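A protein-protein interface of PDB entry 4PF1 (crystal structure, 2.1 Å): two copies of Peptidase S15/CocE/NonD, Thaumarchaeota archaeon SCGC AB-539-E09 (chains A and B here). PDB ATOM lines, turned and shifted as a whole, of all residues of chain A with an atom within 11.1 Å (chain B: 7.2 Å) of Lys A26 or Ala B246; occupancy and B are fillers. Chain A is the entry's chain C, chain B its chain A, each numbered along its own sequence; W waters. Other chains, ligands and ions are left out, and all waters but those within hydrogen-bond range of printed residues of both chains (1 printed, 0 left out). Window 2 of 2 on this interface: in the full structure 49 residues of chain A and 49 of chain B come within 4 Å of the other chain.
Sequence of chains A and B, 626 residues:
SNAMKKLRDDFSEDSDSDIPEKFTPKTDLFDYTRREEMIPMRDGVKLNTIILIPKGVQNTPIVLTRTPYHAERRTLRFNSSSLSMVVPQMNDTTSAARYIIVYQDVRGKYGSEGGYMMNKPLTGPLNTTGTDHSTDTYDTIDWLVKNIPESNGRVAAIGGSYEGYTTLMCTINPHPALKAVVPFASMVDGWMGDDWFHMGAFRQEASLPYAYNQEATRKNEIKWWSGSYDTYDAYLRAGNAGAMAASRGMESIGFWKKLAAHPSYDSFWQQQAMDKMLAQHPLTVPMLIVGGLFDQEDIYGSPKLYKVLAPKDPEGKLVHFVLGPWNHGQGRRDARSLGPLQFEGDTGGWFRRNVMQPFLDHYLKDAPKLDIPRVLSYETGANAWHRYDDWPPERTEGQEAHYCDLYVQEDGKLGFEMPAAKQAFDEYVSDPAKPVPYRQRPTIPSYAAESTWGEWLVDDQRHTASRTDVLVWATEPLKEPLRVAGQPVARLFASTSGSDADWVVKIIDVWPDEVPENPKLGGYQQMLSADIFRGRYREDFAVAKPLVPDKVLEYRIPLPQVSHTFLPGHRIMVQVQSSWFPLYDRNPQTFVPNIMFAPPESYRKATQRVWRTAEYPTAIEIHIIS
OH of Tyr B212 touches CE2 of Phe A23, 3.4 Å away. O of Arg B248 touches CZ of Phe A23, 3.9 Å away. Gly B249 touches Phe A23. Pro A25 touches Tyr B212. Trp B225 touches Lys A26 (NE1 to O, 3.6 Å). Lys A26 touches Ala B246 (CD to O, 3.3 Å). Lys A26 touches Ser B247. Lys A26 touches Arg B248 (CB to C, 3.8 Å). CE2 of Trp B225 touches CE1 of Phe A30 (3.5 Å). Ser A81 touches Trp B225 (CB to CZ3, 3.8 Å).
NH2 of Arg B248 is in hydrogen-bond range of O of Trp B225 (2.8 Å). NZ of Lys A26 is in salt-bridge range of OD1 of Asp A28, 2.8 Å away. The side-chain hydroxyl (OG) of Ser B247 is in hydrogen-bond range of the guanidinium group (NH1) of Arg B248 (3.2 Å). N of Asp A31 sits at hydrogen-bond distance from O of Ser A81 (3.3 Å). NZ of Lys A55 sits at hydrogen-bond distance from O of Phe A30 (3.3 Å). O of Ala B243 lies close to OG of Ser B247.
Water W1 lies within hydrogen-bond range of O of Arg B248 (2.7 Å), OH of Tyr B212 (2.7 Å), N of Lys A26 (2.8 Å) and NE1 of Trp B225 (2.9 Å).
No position is printed for both chains. Of the 12 pairs that touch across the chains among the printed residues, none has its exchanged pair printed and touching as well.
Printed residues of chain B within 4 Å of Lys A26: Trp B225, Ala B246, Ser B247, Arg B248 and Gly B249. Leu A29 touches none of the printed residues of chain B. Of the printed residues of chain B, Asn A79 touches Trp B225 (3.4 Å). Of the printed residues of chain B, Ser A81 touches Trp B225. Leu B208 touches none of the printed residues of chain A. Of the printed residues of chain A, Tyr B212 touches Phe A23 (3.4 Å) and Pro A25 (3.7 Å). No residue of chain A comes within 4 Å of Gly B242. No residue of chain A comes within 4 Å of Ala B243. Ala B246 touches just one residue of chain A: Lys A26 (3.3 Å). Of chain A, only Lys A26 comes within 4 Å of Ser B247. The nearest residue of chain B that does not touch Lys A26 is Tyr B212 (4.9 Å). The nearest residue of chain A that does not touch Ala B246 is Asp A28 (6.8 Å). The nearest printed residue of chain B that does not touch Asn A79 is Tyr B212 (6.4 Å).
Printed residues of chain B that touch a printed residue of chain A: Tyr B212, Trp B225, Ala B246, Ser B247, Arg B248 and Gly B249. Of the 18 printed residues of chain A, 6 touch a printed residue of chain B. Among the printed residues, 12 pairs touch across the chains. Among the printed residues, no Asp or Glu carboxylate lies within 4 Å of a Lys or Arg side-chain nitrogen of the other chain.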
ATOM      1  N   LYS A  22      30.630   7.609 -17.072  1.00  0.00           N
ATOM      2  CA  LYS A  22      29.567   6.770 -16.522  1.00  0.00           C
ATOM      3  C   LYS A  22      28.422   7.642 -15.994  1.00  0.00           C
ATOM      4  O   LYS A  22      28.613   8.402 -15.039  1.00  0.00           O
ATOM      5  CB  LYS A  22      30.115   5.853 -15.410  1.00  0.00           C
ATOM      6  CG  LYS A  22      29.099   4.836 -14.877  1.00  0.00           C
ATOM      7  CD  LYS A  22      29.591   4.138 -13.606  1.00  0.00           C
ATOM      8  CE  LYS A  22      29.208   4.881 -12.344  1.00  0.00           C
ATOM      9  NZ  LYS A  22      29.737   4.211 -11.127  1.00  0.00           N
ATOM     10  N   PHE A  23      27.236   7.534 -16.616  1.00  0.00           N
ATOM     11  CA  PHE A  23      26.073   8.282 -16.159  1.00  0.00           C
ATOM     12  C   PHE A  23      25.157   7.392 -15.329  1.00  0.00           C
ATOM     13  O   PHE A  23      24.906   6.240 -15.688  1.00  0.00           O
ATOM     14  CB  PHE A  23      25.295   8.913 -17.333  1.00  0.00           C
ATOM     15  CG  PHE A  23      24.272   9.939 -16.889  1.00  0.00           C
ATOM     16  CD1 PHE A  23      24.650  11.246 -16.602  1.00  0.00           C
ATOM     17  CD2 PHE A  23      22.935   9.588 -16.728  1.00  0.00           C
ATOM     18  CE1 PHE A  23      23.713  12.182 -16.159  1.00  0.00           C
ATOM     19  CE2 PHE A  23      21.996  10.528 -16.290  1.00  0.00           C
ATOM     20  CZ  PHE A  23      22.390  11.819 -16.013  1.00  0.00           C
ATOM     21  N   THR A  24      24.665   7.933 -14.216  1.00  0.00           N
ATOM     22  CA  THR A  24      23.731   7.246 -13.334  1.00  0.00           C
ATOM     23  C   THR A  24      22.514   8.157 -13.158  1.00  0.00           C
ATOM     24  O   THR A  24      22.655   9.255 -12.607  1.00  0.00           O
ATOM     25  CB  THR A  24      24.411   6.877 -11.991  1.00  0.00           C
ATOM     26  OG1 THR A  24      25.581   6.099 -12.250  1.00  0.00           O
ATOM     27  CG2 THR A  24      23.484   6.103 -11.056  1.00  0.00           C
ATOM     28  N   PRO A  25      21.313   7.749 -13.649  1.00  0.00           N
ATOM     29  CA  PRO A  25      20.129   8.612 -13.486  1.00  0.00           C
ATOM     30  C   PRO A  25      19.812   8.880 -12.012  1.00  0.00           C
ATOM     31  O   PRO A  25      20.124   8.052 -11.146  1.00  0.00           O
ATOM     32  CB  PRO A  25      19.010   7.826 -14.174  1.00  0.00           C
ATOM     33  CG  PRO A  25      19.496   6.423 -14.233  1.00  0.00           C
ATOM     34  CD  PRO A  25      20.976   6.496 -14.357  1.00  0.00           C
ATOM     35  N   LYS A  26      19.251  10.069 -11.730  1.00  0.00           N
ATOM     36  CA  LYS A  26      18.898  10.504 -10.382  1.00  0.00           C
ATOM     37  C   LYS A  26      17.513   9.965 -10.035  1.00  0.00           C
ATOM     38  O   LYS A  26      16.515  10.399 -10.621  1.00  0.00           O
ATOM     39  CB  LYS A  26      18.953  12.037 -10.290  1.00  0.00           C
ATOM     40  CG  LYS A  26      18.812  12.569  -8.883  1.00  0.00           C
ATOM     41  CD  LYS A  26      19.047  14.059  -8.825  1.00  0.00           C
ATOM     42  CE  LYS A  26      18.335  14.708  -7.663  1.00  0.00           C
ATOM     43  NZ  LYS A  26      18.995  14.406  -6.365  1.00  0.00           N
ATOM     44  N   THR A  27      17.458   8.988  -9.114  1.00  0.00           N
ATOM     45  CA  THR A  27      16.211   8.301  -8.769  1.00  0.00           C
ATOM     46  C   THR A  27      15.807   8.430  -7.279  1.00  0.00           C
ATOM     47  O   THR A  27      14.988   7.634  -6.818  1.00  0.00           O
ATOM     48  CB  THR A  27      16.306   6.810  -9.160  1.00  0.00           C
ATOM     49  OG1 THR A  27      17.399   6.210  -8.461  1.00  0.00           O
ATOM     50  CG2 THR A  27      16.468   6.602 -10.659  1.00  0.00           C
ATOM     51  N   ASP A  28      16.321   9.441  -6.543  1.00  0.00           N
ATOM     52  CA  ASP A  28      15.947   9.579  -5.127  1.00  0.00           C
ATOM     53  C   ASP A  28      14.520  10.162  -4.944  1.00  0.00           C
ATOM     54  O   ASP A  28      13.933   9.977  -3.874  1.00  0.00           O
ATOM     55  CB  ASP A  28      16.990  10.370  -4.311  1.00  0.00           C
ATOM     56  CG  ASP A  28      17.338  11.732  -4.860  1.00  0.00           C
ATOM     57  OD1 ASP A  28      18.120  11.795  -5.826  1.00  0.00           O
ATOM     58  OD2 ASP A  28      16.905  12.740  -4.261  1.00  0.00           O
ATOM     59  N   LEU A  29      13.941  10.795  -5.994  1.00  0.00           N
ATOM     60  CA  LEU A  29      12.555  11.297  -5.947  1.00  0.00           C
ATOM     61  C   LEU A  29      11.551  10.195  -6.367  1.00  0.00           C
ATOM     62  O   LEU A  29      10.340  10.388  -6.239  1.00  0.00           O
ATOM     63  CB  LEU A  29      12.361  12.550  -6.839  1.00  0.00           C
ATOM     64  CG  LEU A  29      12.856  13.906  -6.294  1.00  0.00           C
ATOM     65  CD1 LEU A  29      12.676  15.004  -7.340  1.00  0.00           C
ATOM     66  CD2 LEU A  29      12.118  14.309  -5.017  1.00  0.00           C
ATOM     67  N   PHE A  30      12.061   9.053  -6.880  1.00  0.00           N
ATOM     68  CA  PHE A  30      11.247   7.907  -7.313  1.00  0.00           C
ATOM     69  C   PHE A  30      10.652   7.189  -6.095  1.00  0.00           C
ATOM     70  O   PHE A  30      11.291   7.144  -5.043  1.00  0.00           O
ATOM     71  CB  PHE A  30      12.098   6.918  -8.143  1.00  0.00           C
ATOM     72  CG  PHE A  30      12.498   7.347  -9.544  1.00  0.00           C
ATOM     73  CD1 PHE A  30      12.844   8.668  -9.818  1.00  0.00           C
ATOM     74  CD2 PHE A  30      12.611   6.413 -10.567  1.00  0.00           C
ATOM     75  CE1 PHE A  30      13.236   9.055 -11.103  1.00  0.00           C
ATOM     76  CE2 PHE A  30      13.006   6.803 -11.852  1.00  0.00           C
ATOM     77  CZ  PHE A  30      13.318   8.120 -12.110  1.00  0.00           C
ATOM     78  N   ASP A  31       9.445   6.618  -6.238  1.00  0.00           N
ATOM     79  CA  ASP A  31       8.786   5.921  -5.129  1.00  0.00           C
ATOM     80  C   ASP A  31       9.153   4.423  -5.098  1.00  0.00           C
ATOM     81  O   ASP A  31       8.521   3.651  -4.373  1.00  0.00           O
ATOM     82  CB  ASP A  31       7.251   6.123  -5.195  1.00  0.00           C
ATOM     83  CG  ASP A  31       6.529   5.401  -6.330  1.00  0.00           C
ATOM     84  OD1 ASP A  31       7.159   5.164  -7.383  1.00  0.00           O
ATOM     85  OD2 ASP A  31       5.326   5.112  -6.175  1.00  0.00           O
ATOM     86  N   TYR A  32      10.194   4.027  -5.861  1.00  0.00           N
ATOM     87  CA  TYR A  32      10.665   2.643  -5.953  1.00  0.00           C
ATOM     88  C   TYR A  32      12.172   2.575  -6.256  1.00  0.00           C
ATOM     89  O   TYR A  32      12.723   3.494  -6.870  1.00  0.00           O
ATOM     90  CB  TYR A  32       9.875   1.869  -7.040  1.00  0.00           C
ATOM     91  CG  TYR A  32      10.157   2.340  -8.452  1.00  0.00           C
ATOM     92  CD1 TYR A  32       9.554   3.487  -8.959  1.00  0.00           C
ATOM     93  CD2 TYR A  32      11.051   1.657  -9.271  1.00  0.00           C
ATOM     94  CE1 TYR A  32       9.837   3.945 -10.245  1.00  0.00           C
ATOM     95  CE2 TYR A  32      11.353   2.113 -10.554  1.00  0.00           C
ATOM     96  CZ  TYR A  32      10.732   3.251 -11.042  1.00  0.00           C
ATOM     97  OH  TYR A  32      11.008   3.699 -12.311  1.00  0.00           O
ATOM     98  N   THR A  33      12.813   1.455  -5.879  1.00  0.00           N
ATOM     99  CA  THR A  33      14.222   1.187  -6.157  1.00  0.00           C
ATOM    100  C   THR A  33      14.305   0.095  -7.232  1.00  0.00           C
ATOM    101  O   THR A  33      13.670  -0.953  -7.103  1.00  0.00           O
ATOM    102  CB  THR A  33      14.971   0.801  -4.859  1.00  0.00           C
ATOM    103  OG1 THR A  33      14.925   1.904  -3.957  1.00  0.00           O
ATOM    104  CG2 THR A  33      16.429   0.416  -5.106  1.00  0.00           C
ATOM    105  N   ARG A  34      15.072   0.357  -8.292  1.00  0.00           N
ATOM    106  CA  ARG A  34      15.271  -0.580  -9.393  1.00  0.00           C
ATOM    107  C   ARG A  34      16.592  -1.331  -9.187  1.00  0.00           C
ATOM    108  O   ARG A  34      17.667  -0.778  -9.439  1.00  0.00           O
ATOM    109  CB  ARG A  34      15.254   0.180 -10.730  1.00  0.00           C
ATOM    110  CG  ARG A  34      15.364  -0.696 -11.974  1.00  0.00           C
ATOM    111  CD  ARG A  34      15.367   0.159 -13.228  1.00  0.00           C
ATOM    112  NE  ARG A  34      14.098   0.865 -13.404  1.00  0.00           N
ATOM    113  CZ  ARG A  34      13.085   0.406 -14.130  1.00  0.00           C
ATOM    114  NH1 ARG A  34      13.189  -0.755 -14.769  1.00  0.00           N
ATOM    115  NH2 ARG A  34      11.963   1.104 -14.230  1.00  0.00           N
ATOM    116  N   LYS A  55       9.324   1.978  -2.206  1.00  0.00           N
ATOM    117  CA  LYS A  55       9.911   2.670  -1.059  1.00  0.00           C
ATOM    118  C   LYS A  55       8.900   2.752   0.082  1.00  0.00           C
ATOM    119  O   LYS A  55       7.691   2.803  -0.158  1.00  0.00           O
ATOM    120  CB  LYS A  55      10.404   4.070  -1.455  1.00  0.00           C
ATOM    121  CG  LYS A  55      11.696   4.042  -2.255  1.00  0.00           C
ATOM    122  CD  LYS A  55      12.285   5.421  -2.425  1.00  0.00           C
ATOM    123  CE  LYS A  55      13.556   5.379  -3.232  1.00  0.00           C
ATOM    124  NZ  LYS A  55      14.112   6.738  -3.445  1.00  0.00           N
ATOM    125  N   ASN A  79       8.653   5.927 -19.171  1.00  0.00           N
ATOM    126  CA  ASN A  79       9.879   6.329 -18.494  1.00  0.00           C
ATOM    127  C   ASN A  79       9.496   7.276 -17.360  1.00  0.00           C
ATOM    128  O   ASN A  79       9.486   8.497 -17.534  1.00  0.00           O
ATOM    129  CB  ASN A  79      10.858   6.968 -19.482  1.00  0.00           C
ATOM    130  CG  ASN A  79      12.284   6.999 -18.993  1.00  0.00           C
ATOM    131  OD1 ASN A  79      12.604   6.546 -17.891  1.00  0.00           O
ATOM    132  ND2 ASN A  79      13.175   7.524 -19.812  1.00  0.00           N
ATOM    133  N   SER A  80       9.108   6.697 -16.209  1.00  0.00           N
ATOM    134  CA  SER A  80       8.549   7.466 -15.109  1.00  0.00           C
ATOM    135  C   SER A  80       9.232   7.252 -13.756  1.00  0.00           C
ATOM    136  O   SER A  80       9.905   6.246 -13.532  1.00  0.00           O
ATOM    137  CB  SER A  80       7.059   7.150 -14.978  1.00  0.00           C
ATOM    138  OG  SER A  80       6.468   7.726 -13.825  1.00  0.00           O
ATOM    139  N   SER A  81       8.995   8.210 -12.839  1.00  0.00           N
ATOM    140  CA  SER A  81       9.448   8.204 -11.452  1.00  0.00           C
ATOM    141  C   SER A  81       8.455   7.421 -10.560  1.00  0.00           C
ATOM    142  O   SER A  81       8.769   7.127  -9.402  1.00  0.00           O
ATOM    143  CB  SER A  81       9.598   9.636 -10.944  1.00  0.00           C
ATOM    144  OG  SER A  81       8.402  10.376 -11.126  1.00  0.00           O
ATOM    145  N   SER A  82       7.266   7.074 -11.111  1.00  0.00           N
ATOM    146  CA  SER A  82       6.226   6.327 -10.389  1.00  0.00           C
ATOM    147  C   SER A  82       6.206   4.846 -10.783  1.00  0.00           C
ATOM    148  O   SER A  82       6.099   4.531 -11.970  1.00  0.00           O
ATOM    149  CB  SER A  82       4.854   6.945 -10.644  1.00  0.00           C
ATOM    150  OG  SER A  82       4.842   8.306 -10.258  1.00  0.00           O
ATOM    151  N   LEU B 208      16.900  21.116 -22.109  1.00  0.00           N
ATOM    152  CA  LEU B 208      17.183  20.139 -21.044  1.00  0.00           C
ATOM    153  C   LEU B 208      16.919  18.664 -21.455  1.00  0.00           C
ATOM    154  O   LEU B 208      17.857  17.873 -21.355  1.00  0.00           O
ATOM    155  CB  LEU B 208      16.439  20.476 -19.736  1.00  0.00           C
ATOM    156  CG  LEU B 208      16.766  21.828 -19.080  1.00  0.00           C
ATOM    157  CD1 LEU B 208      15.964  22.018 -17.811  1.00  0.00           C
ATOM    158  CD2 LEU B 208      18.247  21.951 -18.766  1.00  0.00           C
ATOM    159  N   TYR B 212      20.050  15.942 -22.241  1.00  0.00           N
ATOM    160  CA  TYR B 212      20.027  14.711 -21.448  1.00  0.00           C
ATOM    161  C   TYR B 212      20.074  13.481 -22.352  1.00  0.00           C
ATOM    162  O   TYR B 212      20.945  12.643 -22.180  1.00  0.00           O
ATOM    163  CB  TYR B 212      18.763  14.674 -20.567  1.00  0.00           C
ATOM    164  CG  TYR B 212      18.757  13.582 -19.519  1.00  0.00           C
ATOM    165  CD1 TYR B 212      18.272  12.310 -19.811  1.00  0.00           C
ATOM    166  CD2 TYR B 212      19.155  13.843 -18.211  1.00  0.00           C
ATOM    167  CE1 TYR B 212      18.227  11.310 -18.839  1.00  0.00           C
ATOM    168  CE2 TYR B 212      19.105  12.856 -17.226  1.00  0.00           C
ATOM    169  CZ  TYR B 212      18.642  11.590 -17.546  1.00  0.00           C
ATOM    170  OH  TYR B 212      18.598  10.612 -16.581  1.00  0.00           O
ATOM    171  N   TRP B 225      13.373  11.072 -17.951  1.00  0.00           N
ATOM    172  CA  TRP B 225      12.216  10.508 -17.267  1.00  0.00           C
ATOM    173  C   TRP B 225      11.218  11.618 -16.908  1.00  0.00           C
ATOM    174  O   TRP B 225      11.595  12.790 -16.826  1.00  0.00           O
ATOM    175  CB  TRP B 225      12.629   9.685 -16.027  1.00  0.00           C
ATOM    176  CG  TRP B 225      13.459  10.430 -15.023  1.00  0.00           C
ATOM    177  CD1 TRP B 225      14.818  10.424 -14.917  1.00  0.00           C
ATOM    178  CD2 TRP B 225      12.975  11.256 -13.953  1.00  0.00           C
ATOM    179  NE1 TRP B 225      15.216  11.215 -13.864  1.00  0.00           N
ATOM    180  CE2 TRP B 225      14.104  11.739 -13.255  1.00  0.00           C
ATOM    181  CE3 TRP B 225      11.694  11.647 -13.523  1.00  0.00           C
ATOM    182  CZ2 TRP B 225      13.993  12.588 -12.147  1.00  0.00           C
ATOM    183  CZ3 TRP B 225      11.585  12.490 -12.428  1.00  0.00           C
ATOM    184  CH2 TRP B 225      12.724  12.947 -11.748  1.00  0.00           C
ATOM    185  N   ALA B 241      15.078  26.728 -14.424  1.00  0.00           N
ATOM    186  CA  ALA B 241      15.670  25.712 -15.305  1.00  0.00           C
ATOM    187  C   ALA B 241      16.791  24.904 -14.613  1.00  0.00           C
ATOM    188  O   ALA B 241      16.967  23.721 -14.916  1.00  0.00           O
ATOM    189  CB  ALA B 241      16.206  26.370 -16.560  1.00  0.00           C
ATOM    190  N   GLY B 242      17.520  25.549 -13.699  1.00  0.00           N
ATOM    191  CA  GLY B 242      18.597  24.925 -12.936  1.00  0.00           C
ATOM    192  C   GLY B 242      18.121  23.808 -12.029  1.00  0.00           C
ATOM    193  O   GLY B 242      18.745  22.744 -11.980  1.00  0.00           O
ATOM    194  N   ALA B 243      16.995  24.030 -11.314  1.00  0.00           N
ATOM    195  CA  ALA B 243      16.420  23.021 -10.416  1.00  0.00           C
ATOM    196  C   ALA B 243      15.824  21.855 -11.205  1.00  0.00           C
ATOM    197  O   ALA B 243      15.764  20.743 -10.688  1.00  0.00           O
ATOM    198  CB  ALA B 243      15.367  23.643  -9.518  1.00  0.00           C
ATOM    199  N   MET B 244      15.389  22.103 -12.460  1.00  0.00           N
ATOM    200  CA  MET B 244      14.864  21.046 -13.323  1.00  0.00           C
ATOM    201  C   MET B 244      16.015  20.150 -13.792  1.00  0.00           C
ATOM    202  O   MET B 244      15.878  18.926 -13.797  1.00  0.00           O
ATOM    203  CB  MET B 244      14.093  21.630 -14.520  1.00  0.00           C
ATOM    204  CG  MET B 244      13.277  20.589 -15.277  1.00  0.00           C
ATOM    205  SD  MET B 244      11.805  20.030 -14.379  1.00  0.00           S
ATOM    206  CE  MET B 244      11.152  18.886 -15.538  1.00  0.00           C
ATOM    207  N   ALA B 245      17.162  20.766 -14.151  1.00  0.00           N
ATOM    208  CA  ALA B 245      18.358  20.050 -14.589  1.00  0.00           C
ATOM    209  C   ALA B 245      18.990  19.273 -13.422  1.00  0.00           C
ATOM    210  O   ALA B 245      19.419  18.136 -13.611  1.00  0.00           O
ATOM    211  CB  ALA B 245      19.362  21.023 -15.184  1.00  0.00           C
ATOM    212  N   ALA B 246      19.002  19.874 -12.214  1.00  0.00           N
ATOM    213  CA  ALA B 246      19.534  19.237 -11.005  1.00  0.00           C
ATOM    214  C   ALA B 246      18.652  18.065 -10.555  1.00  0.00           C
ATOM    215  O   ALA B 246      19.182  17.088 -10.030  1.00  0.00           O
ATOM    216  CB  ALA B 246      19.664  20.254  -9.883  1.00  0.00           C
ATOM    217  N   SER B 247      17.313  18.143 -10.788  1.00  0.00           N
ATOM    218  CA  SER B 247      16.374  17.065 -10.424  1.00  0.00           C
ATOM    219  C   SER B 247      16.608  15.798 -11.281  1.00  0.00           C
ATOM    220  O   SER B 247      16.200  14.706 -10.884  1.00  0.00           O
ATOM    221  CB  SER B 247      14.922  17.534 -10.548  1.00  0.00           C
ATOM    222  OG  SER B 247      14.522  17.704 -11.898  1.00  0.00           O
ATOM    223  N   ARG B 248      17.297  15.949 -12.430  1.00  0.00           N
ATOM    224  CA  ARG B 248      17.624  14.844 -13.334  1.00  0.00           C
ATOM    225  C   ARG B 248      19.115  14.471 -13.255  1.00  0.00           C
ATOM    226  O   ARG B 248      19.553  13.552 -13.952  1.00  0.00           O
ATOM    227  CB  ARG B 248      17.227  15.198 -14.784  1.00  0.00           C
ATOM    228  CG  ARG B 248      15.857  14.657 -15.198  1.00  0.00           C
ATOM    229  CD  ARG B 248      14.724  15.382 -14.504  1.00  0.00           C
ATOM    230  NE  ARG B 248      13.423  15.000 -15.043  1.00  0.00           N
ATOM    231  CZ  ARG B 248      12.264  15.361 -14.507  1.00  0.00           C
ATOM    232  NH1 ARG B 248      12.235  16.092 -13.400  1.00  0.00           N
ATOM    233  NH2 ARG B 248      11.123  14.979 -15.064  1.00  0.00           N
ATOM    234  N   GLY B 249      19.855  15.157 -12.372  1.00  0.00           N
ATOM    235  CA  GLY B 249      21.285  14.943 -12.158  1.00  0.00           C
ATOM    236  C   GLY B 249      22.116  15.239 -13.390  1.00  0.00           C
ATOM    237  O   GLY B 249      22.894  14.390 -13.831  1.00  0.00           O
ATOM    238  N   MET B 250      21.934  16.445 -13.969  1.00  0.00           N
ATOM    239  CA  MET B 250      22.588  16.858 -15.214  1.00  0.00           C
ATOM    240  C   MET B 250      23.877  17.659 -14.986  1.00  0.00           C
ATOM    241  O   MET B 250      24.403  18.245 -15.939  1.00  0.00           O
ATOM    242  CB  MET B 250      21.612  17.685 -16.073  1.00  0.00           C
ATOM    243  CG  MET B 250      20.456  16.878 -16.613  1.00  0.00           C
ATOM    244  SD  MET B 250      19.353  17.835 -17.672  1.00  0.00           S
ATOM    245  CE  MET B 250      20.415  18.102 -19.099  1.00  0.00           C
ATOM    246  N   GLU B 251      24.409  17.652 -13.749  1.00  0.00           N
ATOM    247  CA  GLU B 251      25.630  18.381 -13.389  1.00  0.00           C
ATOM    248  C   GLU B 251      26.860  17.934 -14.208  1.00  0.00           C
ATOM    249  O   GLU B 251      27.741  18.754 -14.458  1.00  0.00           O
ATOM    250  CB  GLU B 251      25.929  18.243 -11.884  1.00  0.00           C
ATOM    251  CG  GLU B 251      24.982  19.039 -10.995  1.00  0.00           C
ATOM    252  CD  GLU B 251      23.692  18.343 -10.587  1.00  0.00           C
ATOM    253  OE1 GLU B 251      23.379  17.272 -11.154  1.00  0.00           O
ATOM    254  OE2 GLU B 251      22.996  18.873  -9.692  1.00  0.00           O
ATOM    255  N   TRP B 256      24.835  21.211 -20.725  1.00  0.00           N
ATOM    256  CA  TRP B 256      24.132  21.932 -19.654  1.00  0.00           C
ATOM    257  C   TRP B 256      25.111  22.854 -18.914  1.00  0.00           C
ATOM    258  O   TRP B 256      24.763  23.997 -18.605  1.00  0.00           O
ATOM    259  CB  TRP B 256      23.431  20.975 -18.665  1.00  0.00           C
ATOM    260  CG  TRP B 256      23.004  21.641 -17.380  1.00  0.00           C
ATOM    261  CD1 TRP B 256      23.457  21.360 -16.125  1.00  0.00           C
ATOM    262  CD2 TRP B 256      22.140  22.784 -17.249  1.00  0.00           C
ATOM    263  NE1 TRP B 256      22.888  22.219 -15.212  1.00  0.00           N
ATOM    264  CE2 TRP B 256      22.089  23.114 -15.877  1.00  0.00           C
ATOM    265  CE3 TRP B 256      21.403  23.562 -18.160  1.00  0.00           C
ATOM    266  CZ2 TRP B 256      21.300  24.163 -15.388  1.00  0.00           C
ATOM    267  CZ3 TRP B 256      20.620  24.600 -17.675  1.00  0.00           C
ATOM    268  CH2 TRP B 256      20.578  24.895 -16.305  1.00  0.00           C
ATOM    269  N   PHE B 597      19.332  29.994 -12.088  1.00  0.00           N
ATOM    270  CA  PHE B 597      19.312  29.674 -10.661  1.00  0.00           C
ATOM    271  C   PHE B 597      18.623  30.780  -9.829  1.00  0.00           C
ATOM    272  O   PHE B 597      18.941  30.946  -8.646  1.00  0.00           O
ATOM    273  CB  PHE B 597      20.758  29.445 -10.155  1.00  0.00           C
ATOM    274  CG  PHE B 597      21.609  28.581 -11.061  1.00  0.00           C
ATOM    275  CD1 PHE B 597      21.454  27.198 -11.078  1.00  0.00           C
ATOM    276  CD2 PHE B 597      22.563  29.150 -11.896  1.00  0.00           C
ATOM    277  CE1 PHE B 597      22.233  26.403 -11.921  1.00  0.00           C
ATOM    278  CE2 PHE B 597      23.345  28.352 -12.736  1.00  0.00           C
ATOM    279  CZ  PHE B 597      23.175  26.984 -12.744  1.00  0.00           C
HETATM  280  O   HOH W   1      18.081  11.319 -13.992  1.00  0.00           O
